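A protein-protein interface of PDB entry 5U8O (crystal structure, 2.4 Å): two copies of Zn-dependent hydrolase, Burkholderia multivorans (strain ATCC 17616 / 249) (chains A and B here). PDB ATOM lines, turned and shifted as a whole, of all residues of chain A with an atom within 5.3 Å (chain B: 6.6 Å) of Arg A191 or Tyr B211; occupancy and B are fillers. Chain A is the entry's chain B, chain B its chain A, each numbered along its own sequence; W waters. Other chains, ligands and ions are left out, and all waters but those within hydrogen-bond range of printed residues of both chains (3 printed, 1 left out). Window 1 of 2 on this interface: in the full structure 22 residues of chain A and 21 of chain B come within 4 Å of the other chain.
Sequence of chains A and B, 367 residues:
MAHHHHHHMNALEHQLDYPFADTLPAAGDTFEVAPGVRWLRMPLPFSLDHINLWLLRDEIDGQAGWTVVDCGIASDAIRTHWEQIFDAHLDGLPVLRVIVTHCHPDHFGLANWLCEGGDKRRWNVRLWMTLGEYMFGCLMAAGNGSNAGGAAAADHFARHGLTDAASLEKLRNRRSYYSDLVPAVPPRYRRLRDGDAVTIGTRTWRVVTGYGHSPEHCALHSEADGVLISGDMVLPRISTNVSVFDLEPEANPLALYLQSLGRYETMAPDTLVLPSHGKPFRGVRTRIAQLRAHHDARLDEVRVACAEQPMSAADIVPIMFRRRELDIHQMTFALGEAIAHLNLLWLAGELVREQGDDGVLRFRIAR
The backbone carbonyl oxygen of Pro B215 is in hydrogen-bond range of the guanidinium group of Arg A191, at 3.1 Å.
O of Leu B256 sits at hydrogen-bond distance from OG of Ser B260 (3.1 Å). OG of Ser B260 is in hydrogen-bond range of N of Tyr B211, at 2.9 Å. The side-chain carboxylate (OD2) of Asp A196 sits at hydrogen-bond distance from the backbone NH (N) of Arg A193 (2.8 Å).
Leu A131 touches Pro B215. Tyr A189 touches Glu B248 (O to CG, 3.3 Å). NH2 of Arg A191 touches CD1 of Tyr B211, at 3.6 Å. Arg A191 touches Glu B248. NH2 of Arg A193 touches CD2 of Tyr B211, at 3.2 Å. Arg A193 touches Leu B256 (NH1 to CD2, 3.1 Å).
Printed residues of chain B within 4 Å of Tyr A189: Glu B248 (3.3 Å). Arg A191 touches just these residues of chain B: Tyr B211 (3.6 Å), Pro B215 (3.1 Å) and Glu B248 (3.1 Å). Of the printed residues of chain B, Arg A193 touches Tyr B211 (3.2 Å) and Leu B256 (3.1 Å). Thr B209 touches none of the printed residues of chain A. Of chain A, only Arg A191 and Arg A193 come within 4 Å of Tyr B211. Of the printed residues of chain A, Pro B215 touches Leu A131 and Arg A191. Of the printed residues of chain A, Glu B248 touches Tyr A189 and Arg A191. The nearest printed residue of chain A that does not touch Tyr B211 is Leu A131 (7.0 Å).
Of the 9 printed residues of chain A, 4 touch a printed residue of chain B. Hydrophobic or aromatic side chains of chain A that line the printed part of chain B: Leu A131 and Tyr A189. Among the printed residues, 7 pairs touch across the chains.
No position is printed for both chains.
Water W1 bridges OE2 of Glu B248 (2.5 Å) and N of Arg A191 (2.9 Å). Water W2 lies within hydrogen-bond range of the backbone carbonyl oxygen of Ser B214, the guanidinium group of Arg A191, the backbone NH of Gly B212 and the backbone carbonyl oxygen of Pro B215. Water W3 bridges OE2 of Glu B248 (3.0 Å) and NH1 of Arg A191 (3.1 Å).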
ATOM      1  N   MET A 129      36.843  30.274 -24.845  1.00  0.00           N
ATOM      2  CA  MET A 129      37.334  28.958 -24.463  1.00  0.00           C
ATOM      3  C   MET A 129      36.145  28.064 -24.092  1.00  0.00           C
ATOM      4  O   MET A 129      35.089  28.551 -23.687  1.00  0.00           O
ATOM      5  CB  MET A 129      38.319  29.110 -23.294  1.00  0.00           C
ATOM      6  CG  MET A 129      39.317  27.985 -23.103  1.00  0.00           C
ATOM      7  SD  MET A 129      40.707  28.589 -22.120  1.00  0.00           S
ATOM      8  CE  MET A 129      41.780  27.161 -22.063  1.00  0.00           C
ATOM      9  N   THR A 130      36.327  26.750 -24.208  1.00  0.00           N
ATOM     10  CA  THR A 130      35.312  25.843 -23.684  1.00  0.00           C
ATOM     11  C   THR A 130      35.431  25.797 -22.164  1.00  0.00           C
ATOM     12  O   THR A 130      36.506  26.029 -21.599  1.00  0.00           O
ATOM     13  CB  THR A 130      35.459  24.415 -24.228  1.00  0.00           C
ATOM     14  OG1 THR A 130      36.670  23.844 -23.730  1.00  0.00           O
ATOM     15  CG2 THR A 130      35.457  24.373 -25.744  1.00  0.00           C
ATOM     16  N   LEU A 131      34.307  25.489 -21.503  1.00  0.00           N
ATOM     17  CA  LEU A 131      34.280  25.479 -20.041  1.00  0.00           C
ATOM     18  C   LEU A 131      35.250  24.445 -19.492  1.00  0.00           C
ATOM     19  O   LEU A 131      35.966  24.715 -18.523  1.00  0.00           O
ATOM     20  CB  LEU A 131      32.853  25.218 -19.528  1.00  0.00           C
ATOM     21  CG  LEU A 131      32.576  25.168 -18.006  1.00  0.00           C
ATOM     22  CD1 LEU A 131      31.148  25.620 -17.629  1.00  0.00           C
ATOM     23  CD2 LEU A 131      32.894  23.797 -17.403  1.00  0.00           C
ATOM     24  N   TYR A 189      35.927  34.531 -18.949  1.00  0.00           N
ATOM     25  CA  TYR A 189      35.971  33.909 -20.269  1.00  0.00           C
ATOM     26  C   TYR A 189      34.595  33.957 -20.914  1.00  0.00           C
ATOM     27  O   TYR A 189      33.574  34.200 -20.251  1.00  0.00           O
ATOM     28  CB  TYR A 189      36.507  32.460 -20.215  1.00  0.00           C
ATOM     29  CG  TYR A 189      35.514  31.375 -19.841  1.00  0.00           C
ATOM     30  CD1 TYR A 189      34.865  31.394 -18.617  1.00  0.00           C
ATOM     31  CD2 TYR A 189      35.274  30.301 -20.694  1.00  0.00           C
ATOM     32  CE1 TYR A 189      33.957  30.391 -18.260  1.00  0.00           C
ATOM     33  CE2 TYR A 189      34.381  29.274 -20.339  1.00  0.00           C
ATOM     34  CZ  TYR A 189      33.724  29.341 -19.128  1.00  0.00           C
ATOM     35  OH  TYR A 189      32.839  28.360 -18.768  1.00  0.00           O
ATOM     36  N   ARG A 190      34.603  33.761 -22.236  1.00  0.00           N
ATOM     37  CA  ARG A 190      33.405  33.567 -23.046  1.00  0.00           C
ATOM     38  C   ARG A 190      33.361  32.101 -23.477  1.00  0.00           C
ATOM     39  O   ARG A 190      34.303  31.607 -24.107  1.00  0.00           O
ATOM     40  CB  ARG A 190      33.395  34.499 -24.256  1.00  0.00           C
ATOM     41  CG  ARG A 190      32.218  34.292 -25.192  1.00  0.00           C
ATOM     42  CD  ARG A 190      31.071  35.208 -24.852  1.00  0.00           C
ATOM     43  NE  ARG A 190      30.005  35.131 -25.848  1.00  0.00           N
ATOM     44  CZ  ARG A 190      29.614  36.148 -26.615  1.00  0.00           C
ATOM     45  NH1 ARG A 190      30.192  37.340 -26.510  1.00  0.00           N
ATOM     46  NH2 ARG A 190      28.634  35.968 -27.490  1.00  0.00           N
ATOM     47  N   ARG A 191      32.270  31.417 -23.138  1.00  0.00           N
ATOM     48  CA  ARG A 191      32.201  29.966 -23.269  1.00  0.00           C
ATOM     49  C   ARG A 191      31.876  29.546 -24.698  1.00  0.00           C
ATOM     50  O   ARG A 191      30.919  30.036 -25.302  1.00  0.00           O
ATOM     51  CB  ARG A 191      31.162  29.403 -22.295  1.00  0.00           C
ATOM     52  CG  ARG A 191      31.040  27.898 -22.288  1.00  0.00           C
ATOM     53  CD  ARG A 191      29.912  27.457 -21.378  1.00  0.00           C
ATOM     54  NE  ARG A 191      29.822  26.002 -21.272  1.00  0.00           N
ATOM     55  CZ  ARG A 191      28.948  25.359 -20.502  1.00  0.00           C
ATOM     56  NH1 ARG A 191      28.078  26.037 -19.768  1.00  0.00           N
ATOM     57  NH2 ARG A 191      28.950  24.039 -20.465  1.00  0.00           N
ATOM     58  N   LEU A 192      32.686  28.649 -25.234  1.00  0.00           N
ATOM     59  CA  LEU A 192      32.430  27.975 -26.499  1.00  0.00           C
ATOM     60  C   LEU A 192      31.853  26.586 -26.234  1.00  0.00           C
ATOM     61  O   LEU A 192      32.339  25.861 -25.364  1.00  0.00           O
ATOM     62  CB  LEU A 192      33.733  27.834 -27.296  1.00  0.00           C
ATOM     63  CG  LEU A 192      34.345  29.156 -27.783  1.00  0.00           C
ATOM     64  CD1 LEU A 192      35.740  28.899 -28.285  1.00  0.00           C
ATOM     65  CD2 LEU A 192      33.492  29.855 -28.833  1.00  0.00           C
ATOM     66  N   ARG A 193      30.848  26.199 -27.016  1.00  0.00           N
ATOM     67  CA  ARG A 193      30.312  24.850 -26.940  1.00  0.00           C
ATOM     68  C   ARG A 193      30.206  24.231 -28.325  1.00  0.00           C
ATOM     69  O   ARG A 193      30.064  24.931 -29.332  1.00  0.00           O
ATOM     70  CB  ARG A 193      28.947  24.829 -26.266  1.00  0.00           C
ATOM     71  CG  ARG A 193      29.005  25.240 -24.807  1.00  0.00           C
ATOM     72  CD  ARG A 193      27.615  25.368 -24.199  1.00  0.00           C
ATOM     73  NE  ARG A 193      26.952  24.069 -24.072  1.00  0.00           N
ATOM     74  CZ  ARG A 193      25.761  23.776 -24.593  1.00  0.00           C
ATOM     75  NH1 ARG A 193      25.081  24.685 -25.269  1.00  0.00           N
ATOM     76  NH2 ARG A 193      25.242  22.569 -24.420  1.00  0.00           N
ATOM     77  N   ASP A 196      28.533  25.622 -31.668  1.00  0.00           N
ATOM     78  CA  ASP A 196      28.425  27.077 -31.693  1.00  0.00           C
ATOM     79  C   ASP A 196      28.963  27.641 -33.006  1.00  0.00           C
ATOM     80  O   ASP A 196      29.929  27.130 -33.575  1.00  0.00           O
ATOM     81  CB  ASP A 196      29.185  27.691 -30.514  1.00  0.00           C
ATOM     82  CG  ASP A 196      28.412  27.604 -29.204  1.00  0.00           C
ATOM     83  OD1 ASP A 196      27.242  27.157 -29.214  1.00  0.00           O
ATOM     84  OD2 ASP A 196      28.975  27.983 -28.160  1.00  0.00           O
ATOM     85  N   ASP B 194      27.253  12.845 -21.241  1.00  0.00           N
ATOM     86  CA  ASP B 194      25.930  12.698 -21.828  1.00  0.00           C
ATOM     87  C   ASP B 194      25.823  11.405 -22.624  1.00  0.00           C
ATOM     88  O   ASP B 194      26.672  11.097 -23.459  1.00  0.00           O
ATOM     89  CB  ASP B 194      25.600  13.883 -22.736  1.00  0.00           C
ATOM     90  CG  ASP B 194      24.120  13.917 -23.122  1.00  0.00           C
ATOM     91  OD1 ASP B 194      23.258  14.002 -22.231  1.00  0.00           O
ATOM     92  OD2 ASP B 194      23.804  13.790 -24.317  1.00  0.00           O
ATOM     93  N   THR B 209      22.590  15.180 -19.790  1.00  0.00           N
ATOM     94  CA  THR B 209      23.274  16.397 -19.361  1.00  0.00           C
ATOM     95  C   THR B 209      22.364  17.611 -19.498  1.00  0.00           C
ATOM     96  O   THR B 209      21.578  17.713 -20.444  1.00  0.00           O
ATOM     97  CB  THR B 209      24.545  16.635 -20.183  1.00  0.00           C
ATOM     98  OG1 THR B 209      25.444  15.546 -20.020  1.00  0.00           O
ATOM     99  CG2 THR B 209      25.258  17.841 -19.669  1.00  0.00           C
ATOM    100  N   GLY B 210      22.489  18.544 -18.563  1.00  0.00           N
ATOM    101  CA  GLY B 210      21.730  19.779 -18.623  1.00  0.00           C
ATOM    102  C   GLY B 210      22.612  20.983 -18.373  1.00  0.00           C
ATOM    103  O   GLY B 210      23.561  20.929 -17.592  1.00  0.00           O
ATOM    104  N   TYR B 211      22.273  22.089 -19.046  1.00  0.00           N
ATOM    105  CA  TYR B 211      23.081  23.303 -19.043  1.00  0.00           C
ATOM    106  C   TYR B 211      22.276  24.504 -18.560  1.00  0.00           C
ATOM    107  O   TYR B 211      21.042  24.472 -18.465  1.00  0.00           O
ATOM    108  CB  TYR B 211      23.651  23.571 -20.444  1.00  0.00           C
ATOM    109  CG  TYR B 211      24.467  22.399 -20.927  1.00  0.00           C
ATOM    110  CD1 TYR B 211      25.800  22.238 -20.538  1.00  0.00           C
ATOM    111  CD2 TYR B 211      23.883  21.415 -21.723  1.00  0.00           C
ATOM    112  CE1 TYR B 211      26.540  21.134 -20.956  1.00  0.00           C
ATOM    113  CE2 TYR B 211      24.589  20.321 -22.143  1.00  0.00           C
ATOM    114  CZ  TYR B 211      25.926  20.179 -21.768  1.00  0.00           C
ATOM    115  OH  TYR B 211      26.626  19.061 -22.204  1.00  0.00           O
ATOM    116  N   GLY B 212      23.008  25.572 -18.247  1.00  0.00           N
ATOM    117  CA  GLY B 212      22.393  26.826 -17.865  1.00  0.00           C
ATOM    118  C   GLY B 212      22.277  27.013 -16.370  1.00  0.00           C
ATOM    119  O   GLY B 212      22.497  28.107 -15.847  1.00  0.00           O
ATOM    120  N   HIS B 213      21.914  25.954 -15.661  1.00  0.00           N
ATOM    121  CA  HIS B 213      21.837  26.044 -14.208  1.00  0.00           C
ATOM    122  C   HIS B 213      23.199  25.849 -13.570  1.00  0.00           C
ATOM    123  O   HIS B 213      23.488  26.436 -12.528  1.00  0.00           O
ATOM    124  CB  HIS B 213      20.862  24.999 -13.660  1.00  0.00           C
ATOM    125  CG  HIS B 213      20.894  24.885 -12.167  1.00  0.00           C
ATOM    126  ND1 HIS B 213      20.442  25.885 -11.330  1.00  0.00           N
ATOM    127  CD2 HIS B 213      21.355  23.902 -11.359  1.00  0.00           C
ATOM    128  CE1 HIS B 213      20.602  25.514 -10.073  1.00  0.00           C
ATOM    129  NE2 HIS B 213      21.146  24.312 -10.062  1.00  0.00           N
ATOM    130  N   SER B 214      24.017  24.991 -14.163  1.00  0.00           N
ATOM    131  CA  SER B 214      25.327  24.637 -13.639  1.00  0.00           C
ATOM    132  C   SER B 214      26.158  24.169 -14.820  1.00  0.00           C
ATOM    133  O   SER B 214      25.628  23.978 -15.920  1.00  0.00           O
ATOM    134  CB  SER B 214      25.212  23.546 -12.571  1.00  0.00           C
ATOM    135  OG  SER B 214      24.701  22.361 -13.144  1.00  0.00           O
ATOM    136  N   PRO B 215      27.467  23.978 -14.635  1.00  0.00           N
ATOM    137  CA  PRO B 215      28.324  23.686 -15.808  1.00  0.00           C
ATOM    138  C   PRO B 215      27.882  22.513 -16.681  1.00  0.00           C
ATOM    139  O   PRO B 215      27.883  22.636 -17.919  1.00  0.00           O
ATOM    140  CB  PRO B 215      29.699  23.427 -15.163  1.00  0.00           C
ATOM    141  CG  PRO B 215      29.680  24.269 -13.936  1.00  0.00           C
ATOM    142  CD  PRO B 215      28.273  24.140 -13.408  1.00  0.00           C
ATOM    143  N   GLU B 216      27.536  21.363 -16.072  1.00  0.00           N
ATOM    144  CA  GLU B 216      27.276  20.137 -16.818  1.00  0.00           C
ATOM    145  C   GLU B 216      26.424  19.176 -15.989  1.00  0.00           C
ATOM    146  O   GLU B 216      26.865  18.090 -15.602  1.00  0.00           O
ATOM    147  CB  GLU B 216      28.604  19.499 -17.233  1.00  0.00           C
ATOM    148  CG  GLU B 216      28.504  18.418 -18.255  1.00  0.00           C
ATOM    149  CD  GLU B 216      29.836  17.743 -18.553  1.00  0.00           C
ATOM    150  OE1 GLU B 216      30.897  18.257 -18.129  1.00  0.00           O
ATOM    151  OE2 GLU B 216      29.818  16.691 -19.226  1.00  0.00           O
ATOM    152  N   HIS B 217      25.195  19.584 -15.722  1.00  0.00           N
ATOM    153  CA  HIS B 217      24.333  18.887 -14.776  1.00  0.00           C
ATOM    154  C   HIS B 217      23.998  17.481 -15.273  1.00  0.00           C
ATOM    155  O   HIS B 217      23.581  17.296 -16.420  1.00  0.00           O
ATOM    156  CB  HIS B 217      23.063  19.713 -14.569  1.00  0.00           C
ATOM    157  CG  HIS B 217      22.120  19.155 -13.553  1.00  0.00           C
ATOM    158  ND1 HIS B 217      21.282  18.096 -13.818  1.00  0.00           N
ATOM    159  CD2 HIS B 217      21.857  19.539 -12.279  1.00  0.00           C
ATOM    160  CE1 HIS B 217      20.548  17.844 -12.748  1.00  0.00           C
ATOM    161  NE2 HIS B 217      20.877  18.706 -11.801  1.00  0.00           N
ATOM    162  N   MET B 233      17.174  20.252 -12.338  1.00  0.00           N
ATOM    163  CA  MET B 233      16.733  20.751 -13.643  1.00  0.00           C
ATOM    164  C   MET B 233      15.210  20.801 -13.768  1.00  0.00           C
ATOM    165  O   MET B 233      14.684  21.703 -14.432  1.00  0.00           O
ATOM    166  CB  MET B 233      17.308  19.886 -14.763  1.00  0.00           C
ATOM    167  CG  MET B 233      18.831  20.051 -14.950  1.00  0.00           C
ATOM    168  SD  MET B 233      19.330  21.687 -15.524  1.00  0.00           S
ATOM    169  CE  MET B 233      18.746  21.679 -17.212  1.00  0.00           C
ATOM    170  N   VAL B 242      18.858  30.337 -12.711  1.00  0.00           N
ATOM    171  CA  VAL B 242      19.810  30.613 -13.796  1.00  0.00           C
ATOM    172  C   VAL B 242      20.365  32.012 -13.572  1.00  0.00           C
ATOM    173  O   VAL B 242      19.600  32.983 -13.506  1.00  0.00           O
ATOM    174  CB  VAL B 242      19.196  30.495 -15.208  1.00  0.00           C
ATOM    175  CG1 VAL B 242      18.915  29.054 -15.550  1.00  0.00           C
ATOM    176  CG2 VAL B 242      17.932  31.340 -15.361  1.00  0.00           C
ATOM    177  N   GLU B 248      31.767  34.532 -16.122  1.00  0.00           N
ATOM    178  CA  GLU B 248      31.326  34.407 -17.507  1.00  0.00           C
ATOM    179  C   GLU B 248      30.302  35.494 -17.775  1.00  0.00           C
ATOM    180  O   GLU B 248      29.100  35.225 -17.891  1.00  0.00           O
ATOM    181  CB  GLU B 248      30.756  33.013 -17.770  1.00  0.00           C
ATOM    182  CG  GLU B 248      30.830  32.602 -19.228  1.00  0.00           C
ATOM    183  CD  GLU B 248      29.941  31.411 -19.545  1.00  0.00           C
ATOM    184  OE1 GLU B 248      29.801  30.532 -18.666  1.00  0.00           O
ATOM    185  OE2 GLU B 248      29.371  31.370 -20.662  1.00  0.00           O
ATOM    186  N   ALA B 251      27.556  35.111 -20.445  1.00  0.00           N
ATOM    187  CA  ALA B 251      26.876  33.822 -20.489  1.00  0.00           C
ATOM    188  C   ALA B 251      25.397  33.965 -20.863  1.00  0.00           C
ATOM    189  O   ALA B 251      24.740  34.965 -20.574  1.00  0.00           O
ATOM    190  CB  ALA B 251      26.993  33.118 -19.139  1.00  0.00           C
ATOM    191  N   PRO B 253      22.847  31.610 -19.783  1.00  0.00           N
ATOM    192  CA  PRO B 253      22.343  30.401 -19.100  1.00  0.00           C
ATOM    193  C   PRO B 253      20.862  30.133 -19.337  1.00  0.00           C
ATOM    194  O   PRO B 253      20.473  28.959 -19.406  1.00  0.00           O
ATOM    195  CB  PRO B 253      22.631  30.682 -17.617  1.00  0.00           C
ATOM    196  CG  PRO B 253      22.604  32.167 -17.516  1.00  0.00           C
ATOM    197  CD  PRO B 253      23.203  32.669 -18.816  1.00  0.00           C
ATOM    198  N   LEU B 254      20.028  31.169 -19.497  1.00  0.00           N
ATOM    199  CA  LEU B 254      18.598  30.926 -19.682  1.00  0.00           C
ATOM    200  C   LEU B 254      18.314  30.227 -21.005  1.00  0.00           C
ATOM    201  O   LEU B 254      17.564  29.246 -21.044  1.00  0.00           O
ATOM    202  CB  LEU B 254      17.799  32.225 -19.571  1.00  0.00           C
ATOM    203  CG  LEU B 254      16.281  31.971 -19.692  1.00  0.00           C
ATOM    204  CD1 LEU B 254      15.773  30.975 -18.657  1.00  0.00           C
ATOM    205  CD2 LEU B 254      15.494  33.259 -19.578  1.00  0.00           C
ATOM    206  N   ALA B 255      18.929  30.683 -22.096  1.00  0.00           N
ATOM    207  CA  ALA B 255      18.803  29.957 -23.363  1.00  0.00           C
ATOM    208  C   ALA B 255      19.314  28.530 -23.240  1.00  0.00           C
ATOM    209  O   ALA B 255      18.684  27.588 -23.744  1.00  0.00           O
ATOM    210  CB  ALA B 255      19.560  30.675 -24.471  1.00  0.00           C
ATOM    211  N   LEU B 256      20.470  28.352 -22.593  1.00  0.00           N
ATOM    212  CA  LEU B 256      20.972  27.008 -22.374  1.00  0.00           C
ATOM    213  C   LEU B 256      19.959  26.179 -21.588  1.00  0.00           C
ATOM    214  O   LEU B 256      19.744  25.001 -21.888  1.00  0.00           O
ATOM    215  CB  LEU B 256      22.317  27.052 -21.643  1.00  0.00           C
ATOM    216  CG  LEU B 256      23.506  27.688 -22.389  1.00  0.00           C
ATOM    217  CD1 LEU B 256      24.775  27.631 -21.550  1.00  0.00           C
ATOM    218  CD2 LEU B 256      23.718  27.026 -23.699  1.00  0.00           C
ATOM    219  N   TYR B 257      19.332  26.779 -20.579  1.00  0.00           N
ATOM    220  CA  TYR B 257      18.391  26.037 -19.746  1.00  0.00           C
ATOM    221  C   TYR B 257      17.170  25.615 -20.548  1.00  0.00           C
ATOM    222  O   TYR B 257      16.783  24.441 -20.535  1.00  0.00           O
ATOM    223  CB  TYR B 257      17.984  26.870 -18.533  1.00  0.00           C
ATOM    224  CG  TYR B 257      16.951  26.205 -17.671  1.00  0.00           C
ATOM    225  CD1 TYR B 257      17.269  25.084 -16.903  1.00  0.00           C
ATOM    226  CD2 TYR B 257      15.653  26.714 -17.585  1.00  0.00           C
ATOM    227  CE1 TYR B 257      16.310  24.468 -16.098  1.00  0.00           C
ATOM    228  CE2 TYR B 257      14.695  26.112 -16.776  1.00  0.00           C
ATOM    229  CZ  TYR B 257      15.030  24.985 -16.042  1.00  0.00           C
ATOM    230  OH  TYR B 257      14.091  24.380 -15.242  1.00  0.00           O
ATOM    231  N   LEU B 258      16.571  26.559 -21.280  1.00  0.00           N
ATOM    232  CA  LEU B 258      15.364  26.272 -22.050  1.00  0.00           C
ATOM    233  C   LEU B 258      15.602  25.189 -23.101  1.00  0.00           C
ATOM    234  O   LEU B 258      14.704  24.383 -23.392  1.00  0.00           O
ATOM    235  CB  LEU B 258      14.877  27.565 -22.700  1.00  0.00           C
ATOM    236  CG  LEU B 258      14.366  28.627 -21.725  1.00  0.00           C
ATOM    237  CD1 LEU B 258      14.072  29.934 -22.477  1.00  0.00           C
ATOM    238  CD2 LEU B 258      13.137  28.128 -20.940  1.00  0.00           C
ATOM    239  N   SER B 260      17.934  22.746 -22.798  1.00  0.00           N
ATOM    240  CA  SER B 260      18.144  21.495 -22.081  1.00  0.00           C
ATOM    241  C   SER B 260      16.818  20.860 -21.671  1.00  0.00           C
ATOM    242  O   SER B 260      16.732  19.633 -21.541  1.00  0.00           O
ATOM    243  CB  SER B 260      19.015  21.737 -20.849  1.00  0.00           C
ATOM    244  OG  SER B 260      20.350  22.046 -21.195  1.00  0.00           O
ATOM    245  N   ARG B 263      15.152  17.850 -23.543  1.00  0.00           N
ATOM    246  CA  ARG B 263      15.505  16.460 -23.248  1.00  0.00           C
ATOM    247  C   ARG B 263      14.433  15.746 -22.426  1.00  0.00           C
ATOM    248  O   ARG B 263      14.294  14.525 -22.524  1.00  0.00           O
ATOM    249  CB  ARG B 263      16.842  16.383 -22.501  1.00  0.00           C
ATOM    250  CG  ARG B 263      18.052  17.025 -23.209  1.00  0.00           C
ATOM    251  CD  ARG B 263      18.405  16.332 -24.514  1.00  0.00           C
ATOM    252  NE  ARG B 263      18.684  14.902 -24.378  1.00  0.00           N
ATOM    253  CZ  ARG B 263      19.863  14.383 -24.028  1.00  0.00           C
ATOM    254  NH1 ARG B 263      20.906  15.167 -23.746  1.00  0.00           N
ATOM    255  NH2 ARG B 263      20.000  13.066 -23.955  1.00  0.00           N
ATOM    256  N   TYR B 264      13.716  16.465 -21.566  1.00  0.00           N
ATOM    257  CA  TYR B 264      12.690  15.834 -20.745  1.00  0.00           C
ATOM    258  C   TYR B 264      11.309  15.867 -21.388  1.00  0.00           C
ATOM    259  O   TYR B 264      10.482  15.006 -21.070  1.00  0.00           O
ATOM    260  CB  TYR B 264      12.669  16.483 -19.350  1.00  0.00           C
ATOM    261  CG  TYR B 264      14.070  16.761 -18.865  1.00  0.00           C
ATOM    262  CD1 TYR B 264      14.879  15.728 -18.438  1.00  0.00           C
ATOM    263  CD2 TYR B 264      14.609  18.063 -18.897  1.00  0.00           C
ATOM    264  CE1 TYR B 264      16.182  15.970 -18.041  1.00  0.00           C
ATOM    265  CE2 TYR B 264      15.907  18.321 -18.484  1.00  0.00           C
ATOM    266  CZ  TYR B 264      16.687  17.263 -18.056  1.00  0.00           C
ATOM    267  OH  TYR B 264      17.977  17.480 -17.651  1.00  0.00           O
HETATM  268  O   HOH W   1      29.746  32.815 -22.681  1.00  0.00           O
HETATM  269  O   HOH W   2      26.011  25.279 -18.119  1.00  0.00           O
HETATM  270  O   HOH W   3      27.472  29.084 -20.101  1.00  0.00           O
